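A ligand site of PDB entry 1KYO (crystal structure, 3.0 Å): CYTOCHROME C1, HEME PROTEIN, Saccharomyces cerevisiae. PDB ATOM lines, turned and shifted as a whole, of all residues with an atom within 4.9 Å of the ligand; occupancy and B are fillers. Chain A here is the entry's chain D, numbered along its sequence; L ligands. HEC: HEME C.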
ATOM      1  N   VAL A  35      20.382  18.018  18.343  1.00  0.00           N
ATOM      2  CA  VAL A  35      19.588  18.952  19.150  1.00  0.00           C
ATOM      3  C   VAL A  35      19.827  18.643  20.629  1.00  0.00           C
ATOM      4  O   VAL A  35      19.797  19.553  21.475  1.00  0.00           O
ATOM      5  CB  VAL A  35      18.086  18.834  18.857  1.00  0.00           C
ATOM      6  CG1 VAL A  35      17.333  19.938  19.545  1.00  0.00           C
ATOM      7  CG2 VAL A  35      17.832  18.851  17.388  1.00  0.00           C
ATOM      8  N   VAL A  39      21.817  21.538  22.800  1.00  0.00           N
ATOM      9  CA  VAL A  39      20.891  22.278  23.672  1.00  0.00           C
ATOM     10  C   VAL A  39      20.441  21.609  24.974  1.00  0.00           C
ATOM     11  O   VAL A  39      20.543  22.220  26.040  1.00  0.00           O
ATOM     12  CB  VAL A  39      19.619  22.716  22.924  1.00  0.00           C
ATOM     13  CG1 VAL A  39      18.876  23.776  23.750  1.00  0.00           C
ATOM     14  CG2 VAL A  39      19.956  23.249  21.543  1.00  0.00           C
ATOM     15  N   CYS A  40      19.930  20.378  24.878  1.00  0.00           N
ATOM     16  CA  CYS A  40      19.437  19.635  26.037  1.00  0.00           C
ATOM     17  C   CYS A  40      20.491  19.082  26.992  1.00  0.00           C
ATOM     18  O   CYS A  40      20.320  19.127  28.210  1.00  0.00           O
ATOM     19  CB  CYS A  40      18.581  18.474  25.551  1.00  0.00           C
ATOM     20  SG  CYS A  40      17.339  18.940  24.328  1.00  0.00           S
ATOM     21  N   CYS A  43      21.756  20.201  30.621  1.00  0.00           N
ATOM     22  CA  CYS A  43      20.985  20.022  31.839  1.00  0.00           C
ATOM     23  C   CYS A  43      20.428  18.618  31.984  1.00  0.00           C
ATOM     24  O   CYS A  43      20.013  18.222  33.066  1.00  0.00           O
ATOM     25  CB  CYS A  43      19.791  20.964  31.867  1.00  0.00           C
ATOM     26  SG  CYS A  43      20.194  22.728  31.880  1.00  0.00           S
ATOM     27  N   HIS A  44      20.420  17.861  30.895  1.00  0.00           N
ATOM     28  CA  HIS A  44      19.849  16.528  30.960  1.00  0.00           C
ATOM     29  C   HIS A  44      20.761  15.370  30.649  1.00  0.00           C
ATOM     30  O   HIS A  44      21.426  15.338  29.614  1.00  0.00           O
ATOM     31  CB  HIS A  44      18.623  16.434  30.050  1.00  0.00           C
ATOM     32  CG  HIS A  44      17.447  17.242  30.529  1.00  0.00           C
ATOM     33  ND1 HIS A  44      16.556  16.825  31.492  1.00  0.00           N
ATOM     34  CD2 HIS A  44      16.998  18.455  30.120  1.00  0.00           C
ATOM     35  CE1 HIS A  44      15.619  17.765  31.624  1.00  0.00           C
ATOM     36  NE2 HIS A  44      15.849  18.779  30.806  1.00  0.00           N
ATOM     37  N   ASN A 108      20.154  24.797  38.896  1.00  0.00           N
ATOM     38  CA  ASN A 108      18.801  24.908  38.365  1.00  0.00           C
ATOM     39  C   ASN A 108      17.727  25.497  39.255  1.00  0.00           C
ATOM     40  O   ASN A 108      16.571  25.081  39.187  1.00  0.00           O
ATOM     41  CB  ASN A 108      18.321  23.560  37.826  1.00  0.00           C
ATOM     42  CG  ASN A 108      18.891  23.248  36.451  1.00  0.00           C
ATOM     43  OD1 ASN A 108      18.583  23.941  35.478  1.00  0.00           O
ATOM     44  ND2 ASN A 108      19.713  22.205  36.370  1.00  0.00           N
ATOM     45  N   ALA A 111      15.786  23.003  41.261  1.00  0.00           N
ATOM     46  CA  ALA A 111      15.103  21.945  40.542  1.00  0.00           C
ATOM     47  C   ALA A 111      16.026  20.874  39.941  1.00  0.00           C
ATOM     48  O   ALA A 111      17.207  21.118  39.671  1.00  0.00           O
ATOM     49  CB  ALA A 111      14.222  22.542  39.470  1.00  0.00           C
ATOM     50  N   LEU A 112      15.457  19.703  39.687  1.00  0.00           N
ATOM     51  CA  LEU A 112      16.230  18.600  39.145  1.00  0.00           C
ATOM     52  C   LEU A 112      15.735  18.119  37.769  1.00  0.00           C
ATOM     53  O   LEU A 112      14.618  17.607  37.644  1.00  0.00           O
ATOM     54  CB  LEU A 112      16.243  17.458  40.167  1.00  0.00           C
ATOM     55  CG  LEU A 112      16.722  16.040  39.815  1.00  0.00           C
ATOM     56  CD1 LEU A 112      18.157  16.004  39.265  1.00  0.00           C
ATOM     57  CD2 LEU A 112      16.579  15.202  41.081  1.00  0.00           C
ATOM     58  N   PRO A 113      16.549  18.330  36.718  1.00  0.00           N
ATOM     59  CA  PRO A 113      16.205  17.904  35.363  1.00  0.00           C
ATOM     60  C   PRO A 113      16.289  16.375  35.249  1.00  0.00           C
ATOM     61  O   PRO A 113      17.362  15.776  35.397  1.00  0.00           O
ATOM     62  CB  PRO A 113      17.274  18.583  34.499  1.00  0.00           C
ATOM     63  CG  PRO A 113      17.695  19.755  35.318  1.00  0.00           C
ATOM     64  CD  PRO A 113      17.747  19.176  36.707  1.00  0.00           C
ATOM     65  N   PRO A 114      15.142  15.738  35.017  1.00  0.00           N
ATOM     66  CA  PRO A 114      15.090  14.286  34.904  1.00  0.00           C
ATOM     67  C   PRO A 114      15.971  13.771  33.792  1.00  0.00           C
ATOM     68  O   PRO A 114      16.276  14.477  32.839  1.00  0.00           O
ATOM     69  CB  PRO A 114      13.614  14.027  34.607  1.00  0.00           C
ATOM     70  CG  PRO A 114      13.148  15.296  33.966  1.00  0.00           C
ATOM     71  CD  PRO A 114      13.819  16.330  34.818  1.00  0.00           C
ATOM     72  N   LEU A 116      16.588  11.972  30.636  1.00  0.00           N
ATOM     73  CA  LEU A 116      15.670  11.800  29.509  1.00  0.00           C
ATOM     74  C   LEU A 116      15.691  10.470  28.748  1.00  0.00           C
ATOM     75  O   LEU A 116      15.119  10.381  27.662  1.00  0.00           O
ATOM     76  CB  LEU A 116      15.828  12.988  28.563  1.00  0.00           C
ATOM     77  CG  LEU A 116      15.610  14.347  29.239  1.00  0.00           C
ATOM     78  CD1 LEU A 116      15.882  15.453  28.247  1.00  0.00           C
ATOM     79  CD2 LEU A 116      14.182  14.444  29.754  1.00  0.00           C
ATOM     80  N   ILE A 119      11.935   9.254  29.256  1.00  0.00           N
ATOM     81  CA  ILE A 119      10.966  10.327  29.381  1.00  0.00           C
ATOM     82  C   ILE A 119       9.704  10.144  28.523  1.00  0.00           C
ATOM     83  O   ILE A 119       8.605  10.344  29.004  1.00  0.00           O
ATOM     84  CB  ILE A 119      11.647  11.696  29.159  1.00  0.00           C
ATOM     85  CG1 ILE A 119      10.794  12.813  29.747  1.00  0.00           C
ATOM     86  CG2 ILE A 119      11.974  11.915  27.690  1.00  0.00           C
ATOM     87  CD1 ILE A 119      10.626  12.655  31.228  1.00  0.00           C
ATOM     88  N   ARG A 123       5.673   9.443  30.702  1.00  0.00           N
ATOM     89  CA  ARG A 123       4.675  10.499  30.662  1.00  0.00           C
ATOM     90  C   ARG A 123       3.504  10.133  29.773  1.00  0.00           C
ATOM     91  O   ARG A 123       3.672   9.472  28.747  1.00  0.00           O
ATOM     92  CB  ARG A 123       5.294  11.769  30.111  1.00  0.00           C
ATOM     93  CG  ARG A 123       6.458  12.331  30.901  1.00  0.00           C
ATOM     94  CD  ARG A 123       5.971  12.865  32.230  1.00  0.00           C
ATOM     95  NE  ARG A 123       6.969  13.696  32.889  1.00  0.00           N
ATOM     96  CZ  ARG A 123       8.019  13.230  33.561  1.00  0.00           C
ATOM     97  NH1 ARG A 123       8.858  14.085  34.130  1.00  0.00           N
ATOM     98  NH2 ARG A 123       8.228  11.923  33.673  1.00  0.00           N
ATOM     99  N   TYR A 129       3.158  14.643  24.053  1.00  0.00           N
ATOM    100  CA  TYR A 129       3.340  15.511  25.213  1.00  0.00           C
ATOM    101  C   TYR A 129       4.724  16.157  25.219  1.00  0.00           C
ATOM    102  O   TYR A 129       4.850  17.353  25.446  1.00  0.00           O
ATOM    103  CB  TYR A 129       3.132  14.765  26.521  1.00  0.00           C
ATOM    104  CG  TYR A 129       3.630  15.516  27.733  1.00  0.00           C
ATOM    105  CD1 TYR A 129       2.812  16.441  28.384  1.00  0.00           C
ATOM    106  CD2 TYR A 129       4.926  15.339  28.209  1.00  0.00           C
ATOM    107  CE1 TYR A 129       3.289  17.165  29.473  1.00  0.00           C
ATOM    108  CE2 TYR A 129       5.397  16.055  29.297  1.00  0.00           C
ATOM    109  CZ  TYR A 129       4.584  16.964  29.920  1.00  0.00           C
ATOM    110  OH  TYR A 129       5.050  17.658  31.009  1.00  0.00           O
ATOM    111  N   ILE A 130       5.763  15.358  25.011  1.00  0.00           N
ATOM    112  CA  ILE A 130       7.127  15.903  25.012  1.00  0.00           C
ATOM    113  C   ILE A 130       7.192  17.043  23.993  1.00  0.00           C
ATOM    114  O   ILE A 130       7.587  18.161  24.333  1.00  0.00           O
ATOM    115  CB  ILE A 130       8.205  14.844  24.649  1.00  0.00           C
ATOM    116  CG1 ILE A 130       8.058  13.598  25.511  1.00  0.00           C
ATOM    117  CG2 ILE A 130       9.572  15.408  24.934  1.00  0.00           C
ATOM    118  CD1 ILE A 130       8.313  13.857  26.966  1.00  0.00           C
ATOM    119  N   LEU A 133       5.029  20.130  24.953  1.00  0.00           N
ATOM    120  CA  LEU A 133       5.639  20.844  26.074  1.00  0.00           C
ATOM    121  C   LEU A 133       6.763  21.732  25.569  1.00  0.00           C
ATOM    122  O   LEU A 133       6.883  22.895  25.982  1.00  0.00           O
ATOM    123  CB  LEU A 133       6.195  19.868  27.123  1.00  0.00           C
ATOM    124  CG  LEU A 133       6.874  20.490  28.356  1.00  0.00           C
ATOM    125  CD1 LEU A 133       5.826  20.835  29.423  1.00  0.00           C
ATOM    126  CD2 LEU A 133       7.914  19.523  28.935  1.00  0.00           C
ATOM    127  N   LEU A 134       7.573  21.183  24.692  1.00  0.00           N
ATOM    128  CA  LEU A 134       8.692  21.921  24.117  1.00  0.00           C
ATOM    129  C   LEU A 134       8.255  23.173  23.351  1.00  0.00           C
ATOM    130  O   LEU A 134       8.747  24.263  23.628  1.00  0.00           O
ATOM    131  CB  LEU A 134       9.533  21.017  23.224  1.00  0.00           C
ATOM    132  CG  LEU A 134      10.355  19.927  23.930  1.00  0.00           C
ATOM    133  CD1 LEU A 134      11.100  19.102  22.882  1.00  0.00           C
ATOM    134  CD2 LEU A 134      11.341  20.538  24.909  1.00  0.00           C
ATOM    135  N   PHE A 157       2.156  21.451  30.893  1.00  0.00           N
ATOM    136  CA  PHE A 157       2.660  20.865  32.114  1.00  0.00           C
ATOM    137  C   PHE A 157       1.584  21.022  33.182  1.00  0.00           C
ATOM    138  O   PHE A 157       0.919  22.051  33.230  1.00  0.00           O
ATOM    139  CB  PHE A 157       3.940  21.573  32.556  1.00  0.00           C
ATOM    140  CG  PHE A 157       4.630  20.937  33.721  1.00  0.00           C
ATOM    141  CD1 PHE A 157       5.325  19.744  33.569  1.00  0.00           C
ATOM    142  CD2 PHE A 157       4.617  21.544  34.971  1.00  0.00           C
ATOM    143  CE1 PHE A 157       6.009  19.171  34.647  1.00  0.00           C
ATOM    144  CE2 PHE A 157       5.294  20.977  36.046  1.00  0.00           C
ATOM    145  CZ  PHE A 157       5.990  19.783  35.885  1.00  0.00           C
ATOM    146  N   ILE A 162       6.237  25.436  35.502  1.00  0.00           N
ATOM    147  CA  ILE A 162       7.332  24.514  35.232  1.00  0.00           C
ATOM    148  C   ILE A 162       8.679  25.219  35.441  1.00  0.00           C
ATOM    149  O   ILE A 162       8.859  26.357  35.001  1.00  0.00           O
ATOM    150  CB  ILE A 162       7.219  23.950  33.764  1.00  0.00           C
ATOM    151  CG1 ILE A 162       8.160  22.760  33.552  1.00  0.00           C
ATOM    152  CG2 ILE A 162       7.486  25.037  32.722  1.00  0.00           C
ATOM    153  CD1 ILE A 162       7.972  22.081  32.203  1.00  0.00           C
ATOM    154  N   ALA A 163       9.623  24.554  36.112  1.00  0.00           N
ATOM    155  CA  ALA A 163      10.938  25.136  36.396  1.00  0.00           C
ATOM    156  C   ALA A 163      11.854  25.296  35.184  1.00  0.00           C
ATOM    157  O   ALA A 163      12.828  26.054  35.223  1.00  0.00           O
ATOM    158  CB  ALA A 163      11.624  24.350  37.481  1.00  0.00           C
ATOM    159  N   MET A 164      11.581  24.567  34.119  1.00  0.00           N
ATOM    160  CA  MET A 164      12.392  24.671  32.914  1.00  0.00           C
ATOM    161  C   MET A 164      11.844  25.800  32.048  1.00  0.00           C
ATOM    162  O   MET A 164      10.646  25.867  31.780  1.00  0.00           O
ATOM    163  CB  MET A 164      12.358  23.350  32.132  1.00  0.00           C
ATOM    164  CG  MET A 164      13.095  23.381  30.799  1.00  0.00           C
ATOM    165  SD  MET A 164      13.179  21.775  30.009  1.00  0.00           S
ATOM    166  CE  MET A 164      11.523  21.616  29.307  1.00  0.00           C
ATOM    167  N   VAL A 167      13.801  26.736  25.768  1.00  0.00           N
ATOM    168  CA  VAL A 167      15.164  26.628  25.253  1.00  0.00           C
ATOM    169  C   VAL A 167      15.242  26.562  23.735  1.00  0.00           C
ATOM    170  O   VAL A 167      16.285  26.890  23.160  1.00  0.00           O
ATOM    171  CB  VAL A 167      15.903  25.392  25.834  1.00  0.00           C
ATOM    172  CG1 VAL A 167      15.874  25.430  27.332  1.00  0.00           C
ATOM    173  CG2 VAL A 167      15.266  24.122  25.334  1.00  0.00           C
ATOM    174  N   LEU A 168      14.167  26.139  23.081  1.00  0.00           N
ATOM    175  CA  LEU A 168      14.150  26.031  21.632  1.00  0.00           C
ATOM    176  C   LEU A 168      13.747  27.318  20.909  1.00  0.00           C
ATOM    177  O   LEU A 168      12.633  27.839  21.096  1.00  0.00           O
ATOM    178  CB  LEU A 168      13.278  24.856  21.165  1.00  0.00           C
ATOM    179  CG  LEU A 168      13.942  23.496  21.379  1.00  0.00           C
ATOM    180  CD1 LEU A 168      13.188  22.395  20.631  1.00  0.00           C
ATOM    181  CD2 LEU A 168      15.393  23.561  20.905  1.00  0.00           C
ATOM    182  N   VAL A 190      14.295  16.130  18.311  1.00  0.00           N
ATOM    183  CA  VAL A 190      14.672  15.633  19.657  1.00  0.00           C
ATOM    184  C   VAL A 190      13.675  14.621  20.193  1.00  0.00           C
ATOM    185  O   VAL A 190      14.069  13.614  20.790  1.00  0.00           O
ATOM    186  CB  VAL A 190      14.793  16.726  20.767  1.00  0.00           C
ATOM    187  CG1 VAL A 190      16.250  16.946  21.115  1.00  0.00           C
ATOM    188  CG2 VAL A 190      14.098  18.018  20.381  1.00  0.00           C
ATOM    189  N   LEU A 194      14.508  11.049  21.441  1.00  0.00           N
ATOM    190  CA  LEU A 194      14.177  10.605  22.786  1.00  0.00           C
ATOM    191  C   LEU A 194      13.278   9.371  22.777  1.00  0.00           C
ATOM    192  O   LEU A 194      13.251   8.597  23.732  1.00  0.00           O
ATOM    193  CB  LEU A 194      13.527  11.732  23.581  1.00  0.00           C
ATOM    194  CG  LEU A 194      14.456  12.909  23.873  1.00  0.00           C
ATOM    195  CD1 LEU A 194      13.816  13.803  24.903  1.00  0.00           C
ATOM    196  CD2 LEU A 194      15.787  12.396  24.383  1.00  0.00           C
HETATM  197 FE   HEC L   1      14.544  20.175  30.360  1.00  0.00          FE
HETATM  198  CHA HEC L   1      12.299  19.036  32.773  1.00  0.00           C
HETATM  199  CHB HEC L   1      12.930  18.245  28.051  1.00  0.00           C
HETATM  200  CHC HEC L   1      16.510  21.462  27.908  1.00  0.00           C
HETATM  201  CHD HEC L   1      16.030  22.092  32.710  1.00  0.00           C
HETATM  202  NA  HEC L   1      12.987  18.841  30.432  1.00  0.00           N
HETATM  203  C1A HEC L   1      12.179  18.519  31.504  1.00  0.00           C
HETATM  204  C2A HEC L   1      11.208  17.543  31.106  1.00  0.00           C
HETATM  205  C3A HEC L   1      11.381  17.317  29.790  1.00  0.00           C
HETATM  206  C4A HEC L   1      12.474  18.160  29.365  1.00  0.00           C
HETATM  207  CMA HEC L   1      10.631  16.383  28.846  1.00  0.00           C
HETATM  208  CAA HEC L   1      10.256  16.943  32.053  1.00  0.00           C
HETATM  209  CBA HEC L   1       8.891  17.586  32.046  1.00  0.00           C
HETATM  210  CGA HEC L   1       7.980  16.984  33.093  1.00  0.00           C
HETATM  211  O1A HEC L   1       8.372  17.022  34.295  1.00  0.00           O
HETATM  212  O2A HEC L   1       6.887  16.480  32.727  1.00  0.00           O
HETATM  213  NB  HEC L   1      14.713  19.874  28.389  1.00  0.00           N
HETATM  214  C1B HEC L   1      13.981  19.020  27.604  1.00  0.00           C
HETATM  215  C2B HEC L   1      14.565  18.943  26.294  1.00  0.00           C
HETATM  216  C3B HEC L   1      15.527  19.875  26.236  1.00  0.00           C
HETATM  217  C4B HEC L   1      15.592  20.491  27.529  1.00  0.00           C
HETATM  218  CMB HEC L   1      14.197  17.927  25.207  1.00  0.00           C
HETATM  219  CAB HEC L   1      16.464  20.315  25.106  1.00  0.00           C
HETATM  220  CBB HEC L   1      15.707  21.007  23.976  1.00  0.00           C
HETATM  221  NC  HEC L   1      15.998  21.462  30.325  1.00  0.00           N
HETATM  222  C1C HEC L   1      16.694  21.909  29.214  1.00  0.00           C
HETATM  223  C2C HEC L   1      17.754  22.794  29.645  1.00  0.00           C
HETATM  224  C3C HEC L   1      17.712  22.840  30.997  1.00  0.00           C
HETATM  225  C4C HEC L   1      16.517  22.138  31.404  1.00  0.00           C
HETATM  226  CMC HEC L   1      18.763  23.487  28.740  1.00  0.00           C
HETATM  227  CAC HEC L   1      18.563  23.375  32.093  1.00  0.00           C
HETATM  228  CBC HEC L   1      18.490  24.879  32.018  1.00  0.00           C
HETATM  229  ND  HEC L   1      14.248  20.463  32.362  1.00  0.00           N
HETATM  230  C1D HEC L   1      14.956  21.338  33.151  1.00  0.00           C
HETATM  231  C2D HEC L   1      14.293  21.485  34.432  1.00  0.00           C
HETATM  232  C3D HEC L   1      13.310  20.571  34.474  1.00  0.00           C
HETATM  233  C4D HEC L   1      13.254  19.948  33.173  1.00  0.00           C
HETATM  234  CMD HEC L   1      14.520  22.544  35.481  1.00  0.00           C
HETATM  235  CAD HEC L   1      12.360  20.322  35.678  1.00  0.00           C
HETATM  236  CBD HEC L   1      10.861  20.569  35.407  1.00  0.00           C
HETATM  237  CGD HEC L   1       9.980  20.508  36.668  1.00  0.00           C
HETATM  238  O1D HEC L   1       9.741  19.378  37.158  1.00  0.00           O
HETATM  239  O2D HEC L   1       9.518  21.575  37.133  1.00  0.00           O
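SG of Cys 43 is bonded to CAC of the ligand, 1.8 Å away.
The side-chain sulfur (SG) of Cys 40 is bonded to a carbon (CAB) of the ligand.
NE2 of His 44 is bound to FE of the ligand (2.0 Å).
FE of the ligand is bound by SD of Met 164, 2.1 Å away.
OH of Tyr 129 is in hydrogen-bond range of O2A of the ligand, at 2.8 Å.
The guanidinium group of Arg 123 is in salt-bridge range of an oxygen (O2A) of the ligand.
The backbone NH (N) of Ala 163 is in hydrogen-bond range of an oxygen (O2D) of the ligand (3.2 Å).
Val 39 touches the ligand.
OD1 of Asn 108 touches CAC of the ligand, 3.4 Å away.
CG of Pro 113 touches C1D of the ligand, at 3.8 Å.
Pro 114 touches the ligand.
Ile 119 touches the ligand (CG1 to CMA, 3.7 Å).
Ile 130 touches the ligand (CD1 to CMA, 3.9 Å).
Leu 133 touches the ligand (CD2 to CBA, 3.8 Å).
Leu 134 touches the ligand.
CE1 of Phe 157 touches O1A of the ligand, at 3.2 Å.
CG1 of Ile 162 touches CBD of the ligand (3.9 Å).
CG2 of Val 167 touches CBB of the ligand (3.4 Å).
Hydrophobic or aromatic side chains that line the ligand: His 44, Pro 113, Pro 114, Ile 119, Tyr 129, Ile 130, Leu 133, Leu 134, Phe 157, Ile 162, Ala 163, Met 164 and Val 167.
A ring nitrogen (ND1) of His 44 is in hydrogen-bond range of the backbone carbonyl oxygen (O) of Pro 114 (2.7 Å).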
